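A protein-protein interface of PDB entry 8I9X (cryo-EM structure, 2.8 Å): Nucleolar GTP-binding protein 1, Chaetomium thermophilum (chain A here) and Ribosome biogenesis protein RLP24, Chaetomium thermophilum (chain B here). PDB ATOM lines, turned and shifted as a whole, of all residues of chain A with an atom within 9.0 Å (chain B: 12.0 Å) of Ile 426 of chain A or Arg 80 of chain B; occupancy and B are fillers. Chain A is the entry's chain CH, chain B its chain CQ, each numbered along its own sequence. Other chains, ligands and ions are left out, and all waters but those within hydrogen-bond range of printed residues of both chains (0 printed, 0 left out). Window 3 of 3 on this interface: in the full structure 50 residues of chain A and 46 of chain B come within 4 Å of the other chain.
O of Ile 426 of chain A lies within hydrogen-bond range of NH1 of Arg 80 of chain B (2.9 Å). The backbone carbonyl oxygen of Ile 450 of chain A is in hydrogen-bond range of the guanidinium group of Arg 75 of chain B (3.0 Å).
OD1 of Asn 82 of chain B sits close to OE1 of Glu 84 of chain B, at 2.7 Å. O of Leu 85 of chain B lies within hydrogen-bond range of OG1 of Thr 89 of chain B, 2.7 Å away.
Among the printed residues, merely in contact across the chains: Leu 427 of chain A with Arg 80 of chain B, Leu 427 of chain A with Tyr 81 of chain B, Trp 432 of chain A with Tyr 81 of chain B, Trp 432 of chain A with Asn 82 of chain B, Trp 432 of chain A with Arg 83 of chain B, Trp 432 of chain A with Glu 84 of chain B, Ile 437 of chain A with Tyr 81 of chain B, Ile 437 of chain A with Trp 86 of chain B, Tyr 447 of chain A with Arg 75 of chain B, Tyr 447 of chain A with Trp 86 of chain B, Ile 450 of chain A with Leu 85 of chain B, Ile 450 of chain A with Trp 86 of chain B, Ile 450 of chain A with Thr 89 of chain B and Pro 452 of chain A with Val 79 of chain B.
Of the printed residues of chain B, Ile 426 of chain A touches Arg 80. Of chain A, only Ile 426 (2.9 Å) and Leu 427 (3.9 Å) come within 4 Å of Arg 80 of chain B. Leu 427 of chain A touches two residues of chain B. Val 79 of chain B touches one residue of chain A. Of the printed residues of chain A, Asn 82 of chain B touches Trp 432. Of the printed residues of chain B, Tyr 447 of chain A touches Arg 75 and Trp 86. Of the printed residues of chain B, Ile 450 of chain A touches Arg 75 (3.0 Å), Leu 85 (3.8 Å), Trp 86 (3.4 Å) and Thr 89 (3.5 Å). Of the printed residues of chain A, Glu 84 of chain B touches Trp 432 (3.2 Å). Asn 76 of chain B touches none of the printed residues of chain A. The nearest residue of chain B that does not touch Ile 426 of chain A is Tyr 81 of chain B (6.9 Å). The nearest residue of chain A that does not touch Arg 80 of chain B is Glu 428 of chain A (5.1 Å). The nearest printed residue of chain B that does not touch Pro 452 of chain A is Leu 85 of chain B (4.5 Å).
Hydrophobic or aromatic side chains of chain A that line the printed part of chain B: Ile 426, Leu 427, Trp 432, Ile 437, Tyr 447, Ile 450 and Pro 452. Printed residues of chain B that touch a printed residue of chain A: Arg 75, Val 79, Arg 80, Tyr 81, Asn 82, Arg 83, Glu 84, Leu 85, Trp 86 and Thr 89. Among the printed residues, 16 pairs touch across the chains.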
ATOM      1  N   LEU A 421      -0.246  15.235  24.199  1.00  0.00           N
ATOM      2  CA  LEU A 421      -0.757  15.019  25.545  1.00  0.00           C
ATOM      3  C   LEU A 421      -2.278  15.029  25.613  1.00  0.00           C
ATOM      4  O   LEU A 421      -2.839  14.625  26.636  1.00  0.00           O
ATOM      5  CB  LEU A 421      -0.199  16.080  26.497  1.00  0.00           C
ATOM      6  CG  LEU A 421       1.236  15.870  26.982  1.00  0.00           C
ATOM      7  CD1 LEU A 421       1.693  17.040  27.837  1.00  0.00           C
ATOM      8  CD2 LEU A 421       1.354  14.566  27.749  1.00  0.00           C
ATOM      9  N   ARG A 422      -2.954  15.474  24.557  1.00  0.00           N
ATOM     10  CA  ARG A 422      -4.408  15.527  24.520  1.00  0.00           C
ATOM     11  C   ARG A 422      -5.027  14.369  23.752  1.00  0.00           C
ATOM     12  O   ARG A 422      -6.242  14.361  23.544  1.00  0.00           O
ATOM     13  CB  ARG A 422      -4.874  16.848  23.908  1.00  0.00           C
ATOM     14  CG  ARG A 422      -4.307  18.082  24.571  1.00  0.00           C
ATOM     15  CD  ARG A 422      -5.061  19.312  24.118  1.00  0.00           C
ATOM     16  NE  ARG A 422      -4.606  20.516  24.799  1.00  0.00           N
ATOM     17  CZ  ARG A 422      -5.347  21.601  24.965  1.00  0.00           C
ATOM     18  NH1 ARG A 422      -6.588  21.664  24.514  1.00  0.00           N
ATOM     19  NH2 ARG A 422      -4.829  22.649  25.600  1.00  0.00           N
ATOM     20  N   LYS A 423      -4.224  13.397  23.319  1.00  0.00           N
ATOM     21  CA  LYS A 423      -4.769  12.285  22.548  1.00  0.00           C
ATOM     22  C   LYS A 423      -5.655  11.391  23.403  1.00  0.00           C
ATOM     23  O   LYS A 423      -6.619  10.806  22.896  1.00  0.00           O
ATOM     24  CB  LYS A 423      -3.631  11.477  21.923  1.00  0.00           C
ATOM     25  CG  LYS A 423      -4.087  10.313  21.062  1.00  0.00           C
ATOM     26  CD  LYS A 423      -2.910   9.653  20.365  1.00  0.00           C
ATOM     27  CE  LYS A 423      -2.056   8.873  21.349  1.00  0.00           C
ATOM     28  NZ  LYS A 423      -2.770   7.680  21.881  1.00  0.00           N
ATOM     29  N   ASP A 424      -5.360  11.282  24.696  1.00  0.00           N
ATOM     30  CA  ASP A 424      -6.119  10.441  25.607  1.00  0.00           C
ATOM     31  C   ASP A 424      -7.121  11.228  26.438  1.00  0.00           C
ATOM     32  O   ASP A 424      -7.702  10.677  27.376  1.00  0.00           O
ATOM     33  CB  ASP A 424      -5.171   9.672  26.527  1.00  0.00           C
ATOM     34  CG  ASP A 424      -4.427   8.568  25.804  1.00  0.00           C
ATOM     35  OD1 ASP A 424      -3.631   7.859  26.457  1.00  0.00           O
ATOM     36  OD2 ASP A 424      -4.635   8.408  24.584  1.00  0.00           O
ATOM     37  N   TRP A 425      -7.330  12.504  26.124  1.00  0.00           N
ATOM     38  CA  TRP A 425      -8.305  13.311  26.847  1.00  0.00           C
ATOM     39  C   TRP A 425      -9.708  12.782  26.581  1.00  0.00           C
ATOM     40  O   TRP A 425     -10.177  12.794  25.439  1.00  0.00           O
ATOM     41  CB  TRP A 425      -8.200  14.771  26.424  1.00  0.00           C
ATOM     42  CG  TRP A 425      -7.233  15.568  27.227  1.00  0.00           C
ATOM     43  CD1 TRP A 425      -6.247  15.088  28.035  1.00  0.00           C
ATOM     44  CD2 TRP A 425      -7.161  16.994  27.307  1.00  0.00           C
ATOM     45  NE1 TRP A 425      -5.564  16.127  28.613  1.00  0.00           N
ATOM     46  CE2 TRP A 425      -6.106  17.309  28.182  1.00  0.00           C
ATOM     47  CE3 TRP A 425      -7.886  18.035  26.723  1.00  0.00           C
ATOM     48  CZ2 TRP A 425      -5.756  18.621  28.485  1.00  0.00           C
ATOM     49  CZ3 TRP A 425      -7.541  19.334  27.026  1.00  0.00           C
ATOM     50  CH2 TRP A 425      -6.485  19.618  27.897  1.00  0.00           C
ATOM     51  N   ILE A 426     -10.380  12.320  27.632  1.00  0.00           N
ATOM     52  CA  ILE A 426     -11.735  11.801  27.495  1.00  0.00           C
ATOM     53  C   ILE A 426     -12.743  12.862  27.926  1.00  0.00           C
ATOM     54  O   ILE A 426     -13.068  13.003  29.109  1.00  0.00           O
ATOM     55  CB  ILE A 426     -11.902  10.473  28.263  1.00  0.00           C
ATOM     56  CG1 ILE A 426     -11.520  10.609  29.740  1.00  0.00           C
ATOM     57  CG2 ILE A 426     -11.077   9.375  27.611  1.00  0.00           C
ATOM     58  CD1 ILE A 426     -11.881   9.406  30.574  1.00  0.00           C
ATOM     59  N   LEU A 427     -13.234  13.628  26.957  1.00  0.00           N
ATOM     60  CA  LEU A 427     -14.193  14.687  27.215  1.00  0.00           C
ATOM     61  C   LEU A 427     -15.594  14.238  26.807  1.00  0.00           C
ATOM     62  O   LEU A 427     -15.824  13.086  26.434  1.00  0.00           O
ATOM     63  CB  LEU A 427     -13.785  15.960  26.479  1.00  0.00           C
ATOM     64  CG  LEU A 427     -12.368  16.468  26.748  1.00  0.00           C
ATOM     65  CD1 LEU A 427     -12.124  17.776  26.021  1.00  0.00           C
ATOM     66  CD2 LEU A 427     -12.135  16.632  28.239  1.00  0.00           C
ATOM     67  N   GLU A 428     -16.547  15.165  26.877  1.00  0.00           N
ATOM     68  CA  GLU A 428     -17.916  14.868  26.478  1.00  0.00           C
ATOM     69  C   GLU A 428     -18.021  14.853  24.960  1.00  0.00           C
ATOM     70  O   GLU A 428     -18.403  13.840  24.366  1.00  0.00           O
ATOM     71  CB  GLU A 428     -18.886  15.887  27.079  1.00  0.00           C
ATOM     72  CG  GLU A 428     -20.354  15.538  26.889  1.00  0.00           C
ATOM     73  CD  GLU A 428     -20.939  16.132  25.621  1.00  0.00           C
ATOM     74  OE1 GLU A 428     -20.684  17.325  25.348  1.00  0.00           O
ATOM     75  OE2 GLU A 428     -21.650  15.406  24.895  1.00  0.00           O
ATOM     76  N   ASN A 429     -17.685  15.969  24.326  1.00  0.00           N
ATOM     77  CA  ASN A 429     -17.670  16.036  22.872  1.00  0.00           C
ATOM     78  C   ASN A 429     -16.242  15.802  22.393  1.00  0.00           C
ATOM     79  O   ASN A 429     -15.337  16.545  22.792  1.00  0.00           O
ATOM     80  CB  ASN A 429     -18.198  17.391  22.401  1.00  0.00           C
ATOM     81  CG  ASN A 429     -18.153  17.570  20.885  1.00  0.00           C
ATOM     82  OD1 ASN A 429     -17.238  17.114  20.202  1.00  0.00           O
ATOM     83  ND2 ASN A 429     -19.165  18.246  20.355  1.00  0.00           N
ATOM     84  N   PRO A 430     -15.992  14.792  21.558  1.00  0.00           N
ATOM     85  CA  PRO A 430     -14.622  14.484  21.131  1.00  0.00           C
ATOM     86  C   PRO A 430     -13.939  15.581  20.330  1.00  0.00           C
ATOM     87  O   PRO A 430     -12.711  15.554  20.210  1.00  0.00           O
ATOM     88  CB  PRO A 430     -14.814  13.226  20.267  1.00  0.00           C
ATOM     89  CG  PRO A 430     -16.097  12.635  20.728  1.00  0.00           C
ATOM     90  CD  PRO A 430     -16.962  13.805  21.058  1.00  0.00           C
ATOM     91  N   TRP A 432     -13.809  18.695  21.216  1.00  0.00           N
ATOM     92  CA  TRP A 432     -13.307  19.725  22.114  1.00  0.00           C
ATOM     93  C   TRP A 432     -11.838  19.535  22.458  1.00  0.00           C
ATOM     94  O   TRP A 432     -11.247  20.414  23.092  1.00  0.00           O
ATOM     95  CB  TRP A 432     -14.136  19.763  23.397  1.00  0.00           C
ATOM     96  CG  TRP A 432     -15.544  20.200  23.165  1.00  0.00           C
ATOM     97  CD1 TRP A 432     -16.026  20.840  22.066  1.00  0.00           C
ATOM     98  CD2 TRP A 432     -16.645  20.067  24.067  1.00  0.00           C
ATOM     99  NE1 TRP A 432     -17.364  21.099  22.216  1.00  0.00           N
ATOM    100  CE2 TRP A 432     -17.769  20.633  23.439  1.00  0.00           C
ATOM    101  CE3 TRP A 432     -16.793  19.512  25.340  1.00  0.00           C
ATOM    102  CZ2 TRP A 432     -19.021  20.662  24.038  1.00  0.00           C
ATOM    103  CZ3 TRP A 432     -18.035  19.542  25.933  1.00  0.00           C
ATOM    104  CH2 TRP A 432     -19.135  20.112  25.284  1.00  0.00           C
ATOM    105  N   LYS A 433     -11.246  18.413  22.066  1.00  0.00           N
ATOM    106  CA  LYS A 433      -9.811  18.229  22.191  1.00  0.00           C
ATOM    107  C   LYS A 433      -9.084  19.223  21.293  1.00  0.00           C
ATOM    108  O   LYS A 433      -9.649  19.748  20.329  1.00  0.00           O
ATOM    109  CB  LYS A 433      -9.433  16.800  21.811  1.00  0.00           C
ATOM    110  CG  LYS A 433     -10.017  15.744  22.733  1.00  0.00           C
ATOM    111  CD  LYS A 433     -10.112  14.400  22.031  1.00  0.00           C
ATOM    112  CE  LYS A 433      -8.978  13.475  22.414  1.00  0.00           C
ATOM    113  NZ  LYS A 433      -9.041  12.189  21.668  1.00  0.00           N
ATOM    114  N   ILE A 437      -7.664  26.406  26.088  1.00  0.00           N
ATOM    115  CA  ILE A 437      -8.472  26.751  27.254  1.00  0.00           C
ATOM    116  C   ILE A 437      -8.041  28.116  27.777  1.00  0.00           C
ATOM    117  O   ILE A 437      -6.853  28.321  28.066  1.00  0.00           O
ATOM    118  CB  ILE A 437      -8.355  25.685  28.353  1.00  0.00           C
ATOM    119  CG1 ILE A 437      -8.422  24.283  27.747  1.00  0.00           C
ATOM    120  CG2 ILE A 437      -9.448  25.870  29.390  1.00  0.00           C
ATOM    121  CD1 ILE A 437      -7.977  23.193  28.691  1.00  0.00           C
ATOM    122  N   TYR A 447      -9.802  29.894  35.568  1.00  0.00           N
ATOM    123  CA  TYR A 447      -9.902  28.683  36.370  1.00  0.00           C
ATOM    124  C   TYR A 447     -10.398  28.954  37.781  1.00  0.00           C
ATOM    125  O   TYR A 447     -11.177  28.152  38.307  1.00  0.00           O
ATOM    126  CB  TYR A 447      -8.550  27.973  36.430  1.00  0.00           C
ATOM    127  CG  TYR A 447      -8.334  27.001  35.298  1.00  0.00           C
ATOM    128  CD1 TYR A 447      -8.153  27.450  34.000  1.00  0.00           C
ATOM    129  CD2 TYR A 447      -8.320  25.635  35.526  1.00  0.00           C
ATOM    130  CE1 TYR A 447      -7.956  26.567  32.961  1.00  0.00           C
ATOM    131  CE2 TYR A 447      -8.125  24.743  34.493  1.00  0.00           C
ATOM    132  CZ  TYR A 447      -7.944  25.215  33.213  1.00  0.00           C
ATOM    133  OH  TYR A 447      -7.749  24.332  32.176  1.00  0.00           O
ATOM    134  N   ILE A 450     -14.026  29.173  37.403  1.00  0.00           N
ATOM    135  CA  ILE A 450     -14.720  27.971  36.949  1.00  0.00           C
ATOM    136  C   ILE A 450     -15.426  27.315  38.125  1.00  0.00           C
ATOM    137  O   ILE A 450     -14.795  26.957  39.125  1.00  0.00           O
ATOM    138  CB  ILE A 450     -13.765  26.969  36.273  1.00  0.00           C
ATOM    139  CG1 ILE A 450     -13.169  27.556  34.996  1.00  0.00           C
ATOM    140  CG2 ILE A 450     -14.493  25.672  35.966  1.00  0.00           C
ATOM    141  CD1 ILE A 450     -14.200  27.910  33.952  1.00  0.00           C
ATOM    142  N   PRO A 452     -18.797  24.448  38.407  1.00  0.00           N
ATOM    143  CA  PRO A 452     -19.973  23.762  37.854  1.00  0.00           C
ATOM    144  C   PRO A 452     -21.235  24.236  38.555  1.00  0.00           C
ATOM    145  O   PRO A 452     -21.216  24.571  39.742  1.00  0.00           O
ATOM    146  CB  PRO A 452     -19.686  22.281  38.126  1.00  0.00           C
ATOM    147  CG  PRO A 452     -18.654  22.266  39.198  1.00  0.00           C
ATOM    148  CD  PRO A 452     -17.857  23.523  39.060  1.00  0.00           C
ATOM    149  N   ARG B  75      -9.556  26.852  43.498  1.00  0.00           N
ATOM    150  CA  ARG B  75     -10.233  25.579  43.288  1.00  0.00           C
ATOM    151  C   ARG B  75      -9.231  24.436  43.388  1.00  0.00           C
ATOM    152  O   ARG B  75      -8.265  24.381  42.620  1.00  0.00           O
ATOM    153  CB  ARG B  75     -10.930  25.562  41.929  1.00  0.00           C
ATOM    154  CG  ARG B  75     -11.772  26.793  41.654  1.00  0.00           C
ATOM    155  CD  ARG B  75     -13.103  26.716  42.377  1.00  0.00           C
ATOM    156  NE  ARG B  75     -14.018  27.766  41.951  1.00  0.00           N
ATOM    157  CZ  ARG B  75     -14.383  28.792  42.706  1.00  0.00           C
ATOM    158  NH1 ARG B  75     -13.939  28.931  43.943  1.00  0.00           N
ATOM    159  NH2 ARG B  75     -15.218  29.700  42.209  1.00  0.00           N
ATOM    160  N   ASN B  76      -9.466  23.525  44.330  1.00  0.00           N
ATOM    161  CA  ASN B  76      -8.631  22.347  44.507  1.00  0.00           C
ATOM    162  C   ASN B  76      -9.244  21.090  43.905  1.00  0.00           C
ATOM    163  O   ASN B  76      -8.618  20.026  43.960  1.00  0.00           O
ATOM    164  CB  ASN B  76      -8.350  22.124  45.996  1.00  0.00           C
ATOM    165  CG  ASN B  76      -7.333  23.100  46.546  1.00  0.00           C
ATOM    166  OD1 ASN B  76      -6.803  23.936  45.816  1.00  0.00           O
ATOM    167  ND2 ASN B  76      -7.058  23.005  47.841  1.00  0.00           N
ATOM    168  N   VAL B  77     -10.437  21.181  43.333  1.00  0.00           N
ATOM    169  CA  VAL B  77     -11.119  20.048  42.724  1.00  0.00           C
ATOM    170  C   VAL B  77     -11.357  20.371  41.253  1.00  0.00           C
ATOM    171  O   VAL B  77     -12.158  21.244  40.920  1.00  0.00           O
ATOM    172  CB  VAL B  77     -12.440  19.731  43.445  1.00  0.00           C
ATOM    173  CG1 VAL B  77     -13.159  18.587  42.751  1.00  0.00           C
ATOM    174  CG2 VAL B  77     -12.175  19.395  44.899  1.00  0.00           C
ATOM    175  N   PRO B  78     -10.670  19.685  40.343  1.00  0.00           N
ATOM    176  CA  PRO B  78     -10.764  20.040  38.924  1.00  0.00           C
ATOM    177  C   PRO B  78     -12.128  19.721  38.334  1.00  0.00           C
ATOM    178  O   PRO B  78     -12.870  18.875  38.839  1.00  0.00           O
ATOM    179  CB  PRO B  78      -9.670  19.186  38.275  1.00  0.00           C
ATOM    180  CG  PRO B  78      -9.509  18.031  39.203  1.00  0.00           C
ATOM    181  CD  PRO B  78      -9.709  18.595  40.574  1.00  0.00           C
ATOM    182  N   VAL B  79     -12.453  20.421  37.253  1.00  0.00           N
ATOM    183  CA  VAL B  79     -13.662  20.172  36.483  1.00  0.00           C
ATOM    184  C   VAL B  79     -13.258  19.801  35.061  1.00  0.00           C
ATOM    185  O   VAL B  79     -12.347  20.388  34.470  1.00  0.00           O
ATOM    186  CB  VAL B  79     -14.608  21.389  36.488  1.00  0.00           C
ATOM    187  CG1 VAL B  79     -15.923  21.048  35.806  1.00  0.00           C
ATOM    188  CG2 VAL B  79     -14.844  21.868  37.909  1.00  0.00           C
ATOM    189  N   ARG B  80     -13.945  18.804  34.512  1.00  0.00           N
ATOM    190  CA  ARG B  80     -13.668  18.346  33.158  1.00  0.00           C
ATOM    191  C   ARG B  80     -13.964  19.450  32.149  1.00  0.00           C
ATOM    192  O   ARG B  80     -14.948  20.185  32.274  1.00  0.00           O
ATOM    193  CB  ARG B  80     -14.491  17.100  32.837  1.00  0.00           C
ATOM    194  CG  ARG B  80     -14.007  16.328  31.628  1.00  0.00           C
ATOM    195  CD  ARG B  80     -14.624  14.941  31.581  1.00  0.00           C
ATOM    196  NE  ARG B  80     -14.260  14.161  32.758  1.00  0.00           N
ATOM    197  CZ  ARG B  80     -13.138  13.467  32.878  1.00  0.00           C
ATOM    198  NH1 ARG B  80     -12.244  13.424  31.904  1.00  0.00           N
ATOM    199  NH2 ARG B  80     -12.905  12.802  34.005  1.00  0.00           N
ATOM    200  N   TYR B  81     -13.090  19.568  31.150  1.00  0.00           N
ATOM    201  CA  TYR B  81     -13.153  20.669  30.192  1.00  0.00           C
ATOM    202  C   TYR B  81     -14.496  20.668  29.469  1.00  0.00           C
ATOM    203  O   TYR B  81     -15.041  19.608  29.152  1.00  0.00           O
ATOM    204  CB  TYR B  81     -12.002  20.586  29.197  1.00  0.00           C
ATOM    205  CG  TYR B  81     -12.071  21.658  28.136  1.00  0.00           C
ATOM    206  CD1 TYR B  81     -12.376  21.344  26.822  1.00  0.00           C
ATOM    207  CD2 TYR B  81     -11.859  22.990  28.458  1.00  0.00           C
ATOM    208  CE1 TYR B  81     -12.451  22.324  25.855  1.00  0.00           C
ATOM    209  CE2 TYR B  81     -11.934  23.975  27.499  1.00  0.00           C
ATOM    210  CZ  TYR B  81     -12.230  23.637  26.199  1.00  0.00           C
ATOM    211  OH  TYR B  81     -12.302  24.619  25.239  1.00  0.00           O
ATOM    212  N   ASN B  82     -15.028  21.862  29.216  1.00  0.00           N
ATOM    213  CA  ASN B  82     -16.336  22.049  28.604  1.00  0.00           C
ATOM    214  C   ASN B  82     -16.413  23.454  28.018  1.00  0.00           C
ATOM    215  O   ASN B  82     -16.428  24.444  28.763  1.00  0.00           O
ATOM    216  CB  ASN B  82     -17.439  21.822  29.640  1.00  0.00           C
ATOM    217  CG  ASN B  82     -18.815  21.765  29.027  1.00  0.00           C
ATOM    218  OD1 ASN B  82     -18.970  21.857  27.814  1.00  0.00           O
ATOM    219  ND2 ASN B  82     -19.829  21.605  29.868  1.00  0.00           N
ATOM    220  N   ARG B  83     -16.485  23.537  26.686  1.00  0.00           N
ATOM    221  CA  ARG B  83     -16.402  24.836  26.024  1.00  0.00           C
ATOM    222  C   ARG B  83     -17.534  25.759  26.444  1.00  0.00           C
ATOM    223  O   ARG B  83     -17.313  26.956  26.661  1.00  0.00           O
ATOM    224  CB  ARG B  83     -16.396  24.673  24.505  1.00  0.00           C
ATOM    225  CG  ARG B  83     -15.148  24.032  23.959  1.00  0.00           C
ATOM    226  CD  ARG B  83     -15.230  23.899  22.457  1.00  0.00           C
ATOM    227  NE  ARG B  83     -15.243  25.186  21.779  1.00  0.00           N
ATOM    228  CZ  ARG B  83     -15.456  25.340  20.480  1.00  0.00           C
ATOM    229  NH1 ARG B  83     -15.666  24.302  19.688  1.00  0.00           N
ATOM    230  NH2 ARG B  83     -15.456  26.565  19.962  1.00  0.00           N
ATOM    231  N   GLU B  84     -18.754  25.234  26.549  1.00  0.00           N
ATOM    232  CA  GLU B  84     -19.859  26.062  27.016  1.00  0.00           C
ATOM    233  C   GLU B  84     -19.583  26.580  28.419  1.00  0.00           C
ATOM    234  O   GLU B  84     -19.861  27.744  28.733  1.00  0.00           O
ATOM    235  CB  GLU B  84     -21.171  25.276  26.967  1.00  0.00           C
ATOM    236  CG  GLU B  84     -21.643  24.934  25.563  1.00  0.00           C
ATOM    237  CD  GLU B  84     -20.974  23.701  25.000  1.00  0.00           C
ATOM    238  OE1 GLU B  84     -20.182  23.070  25.726  1.00  0.00           O
ATOM    239  OE2 GLU B  84     -21.239  23.362  23.828  1.00  0.00           O
ATOM    240  N   LEU B  85     -19.000  25.735  29.272  1.00  0.00           N
ATOM    241  CA  LEU B  85     -18.723  26.145  30.643  1.00  0.00           C
ATOM    242  C   LEU B  85     -17.724  27.297  30.688  1.00  0.00           C
ATOM    243  O   LEU B  85     -17.975  28.312  31.341  1.00  0.00           O
ATOM    244  CB  LEU B  85     -18.216  24.954  31.456  1.00  0.00           C
ATOM    245  CG  LEU B  85     -17.868  25.244  32.917  1.00  0.00           C
ATOM    246  CD1 LEU B  85     -19.137  25.437  33.725  1.00  0.00           C
ATOM    247  CD2 LEU B  85     -17.021  24.133  33.511  1.00  0.00           C
ATOM    248  N   TRP B  86     -16.588  27.162  29.995  1.00  0.00           N
ATOM    249  CA  TRP B  86     -15.617  28.261  29.939  1.00  0.00           C
ATOM    250  C   TRP B  86     -16.156  29.526  29.270  1.00  0.00           C
ATOM    251  O   TRP B  86     -15.892  30.636  29.747  1.00  0.00           O
ATOM    252  CB  TRP B  86     -14.312  27.782  29.300  1.00  0.00           C
ATOM    253  CG  TRP B  86     -13.371  27.125  30.283  1.00  0.00           C
ATOM    254  CD1 TRP B  86     -12.330  27.742  30.914  1.00  0.00           C
ATOM    255  CD2 TRP B  86     -13.487  25.834  30.894  1.00  0.00           C
ATOM    256  NE1 TRP B  86     -11.721  26.885  31.787  1.00  0.00           N
ATOM    257  CE2 TRP B  86     -12.420  25.709  31.808  1.00  0.00           C
ATOM    258  CE3 TRP B  86     -14.354  24.758  30.731  1.00  0.00           C
ATOM    259  CZ2 TRP B  86     -12.204  24.555  32.550  1.00  0.00           C
ATOM    260  CZ3 TRP B  86     -14.140  23.618  31.474  1.00  0.00           C
ATOM    261  CH2 TRP B  86     -13.072  23.521  32.366  1.00  0.00           C
ATOM    262  N   GLN B  87     -16.896  29.406  28.165  1.00  0.00           N
ATOM    263  CA  GLN B  87     -17.420  30.617  27.531  1.00  0.00           C
ATOM    264  C   GLN B  87     -18.411  31.338  28.442  1.00  0.00           C
ATOM    265  O   GLN B  87     -18.332  32.566  28.629  1.00  0.00           O
ATOM    266  CB  GLN B  87     -18.072  30.273  26.192  1.00  0.00           C
ATOM    267  CG  GLN B  87     -17.128  29.647  25.181  1.00  0.00           C
ATOM    268  CD  GLN B  87     -15.855  30.449  25.000  1.00  0.00           C
ATOM    269  OE1 GLN B  87     -14.755  29.955  25.246  1.00  0.00           O
ATOM    270  NE2 GLN B  87     -15.999  31.696  24.566  1.00  0.00           N
ATOM    271  N   LYS B  88     -19.350  30.589  29.017  1.00  0.00           N
ATOM    272  CA  LYS B  88     -20.311  31.163  29.945  1.00  0.00           C
ATOM    273  C   LYS B  88     -19.612  31.729  31.174  1.00  0.00           C
ATOM    274  O   LYS B  88     -20.036  32.754  31.720  1.00  0.00           O
ATOM    275  CB  LYS B  88     -21.328  30.088  30.317  1.00  0.00           C
ATOM    276  CG  LYS B  88     -22.431  30.509  31.244  1.00  0.00           C
ATOM    277  CD  LYS B  88     -23.402  29.358  31.383  1.00  0.00           C
ATOM    278  CE  LYS B  88     -22.812  28.244  32.232  1.00  0.00           C
ATOM    279  NZ  LYS B  88     -23.791  27.151  32.481  1.00  0.00           N
ATOM    280  N   THR B  89     -18.518  31.093  31.602  1.00  0.00           N
ATOM    281  CA  THR B  89     -17.739  31.615  32.715  1.00  0.00           C
ATOM    282  C   THR B  89     -17.103  32.949  32.362  1.00  0.00           C
ATOM    283  O   THR B  89     -17.065  33.859  33.190  1.00  0.00           O
ATOM    284  CB  THR B  89     -16.670  30.601  33.126  1.00  0.00           C
ATOM    285  OG1 THR B  89     -17.297  29.454  33.714  1.00  0.00           O
ATOM    286  CG2 THR B  89     -15.708  31.210  34.134  1.00  0.00           C
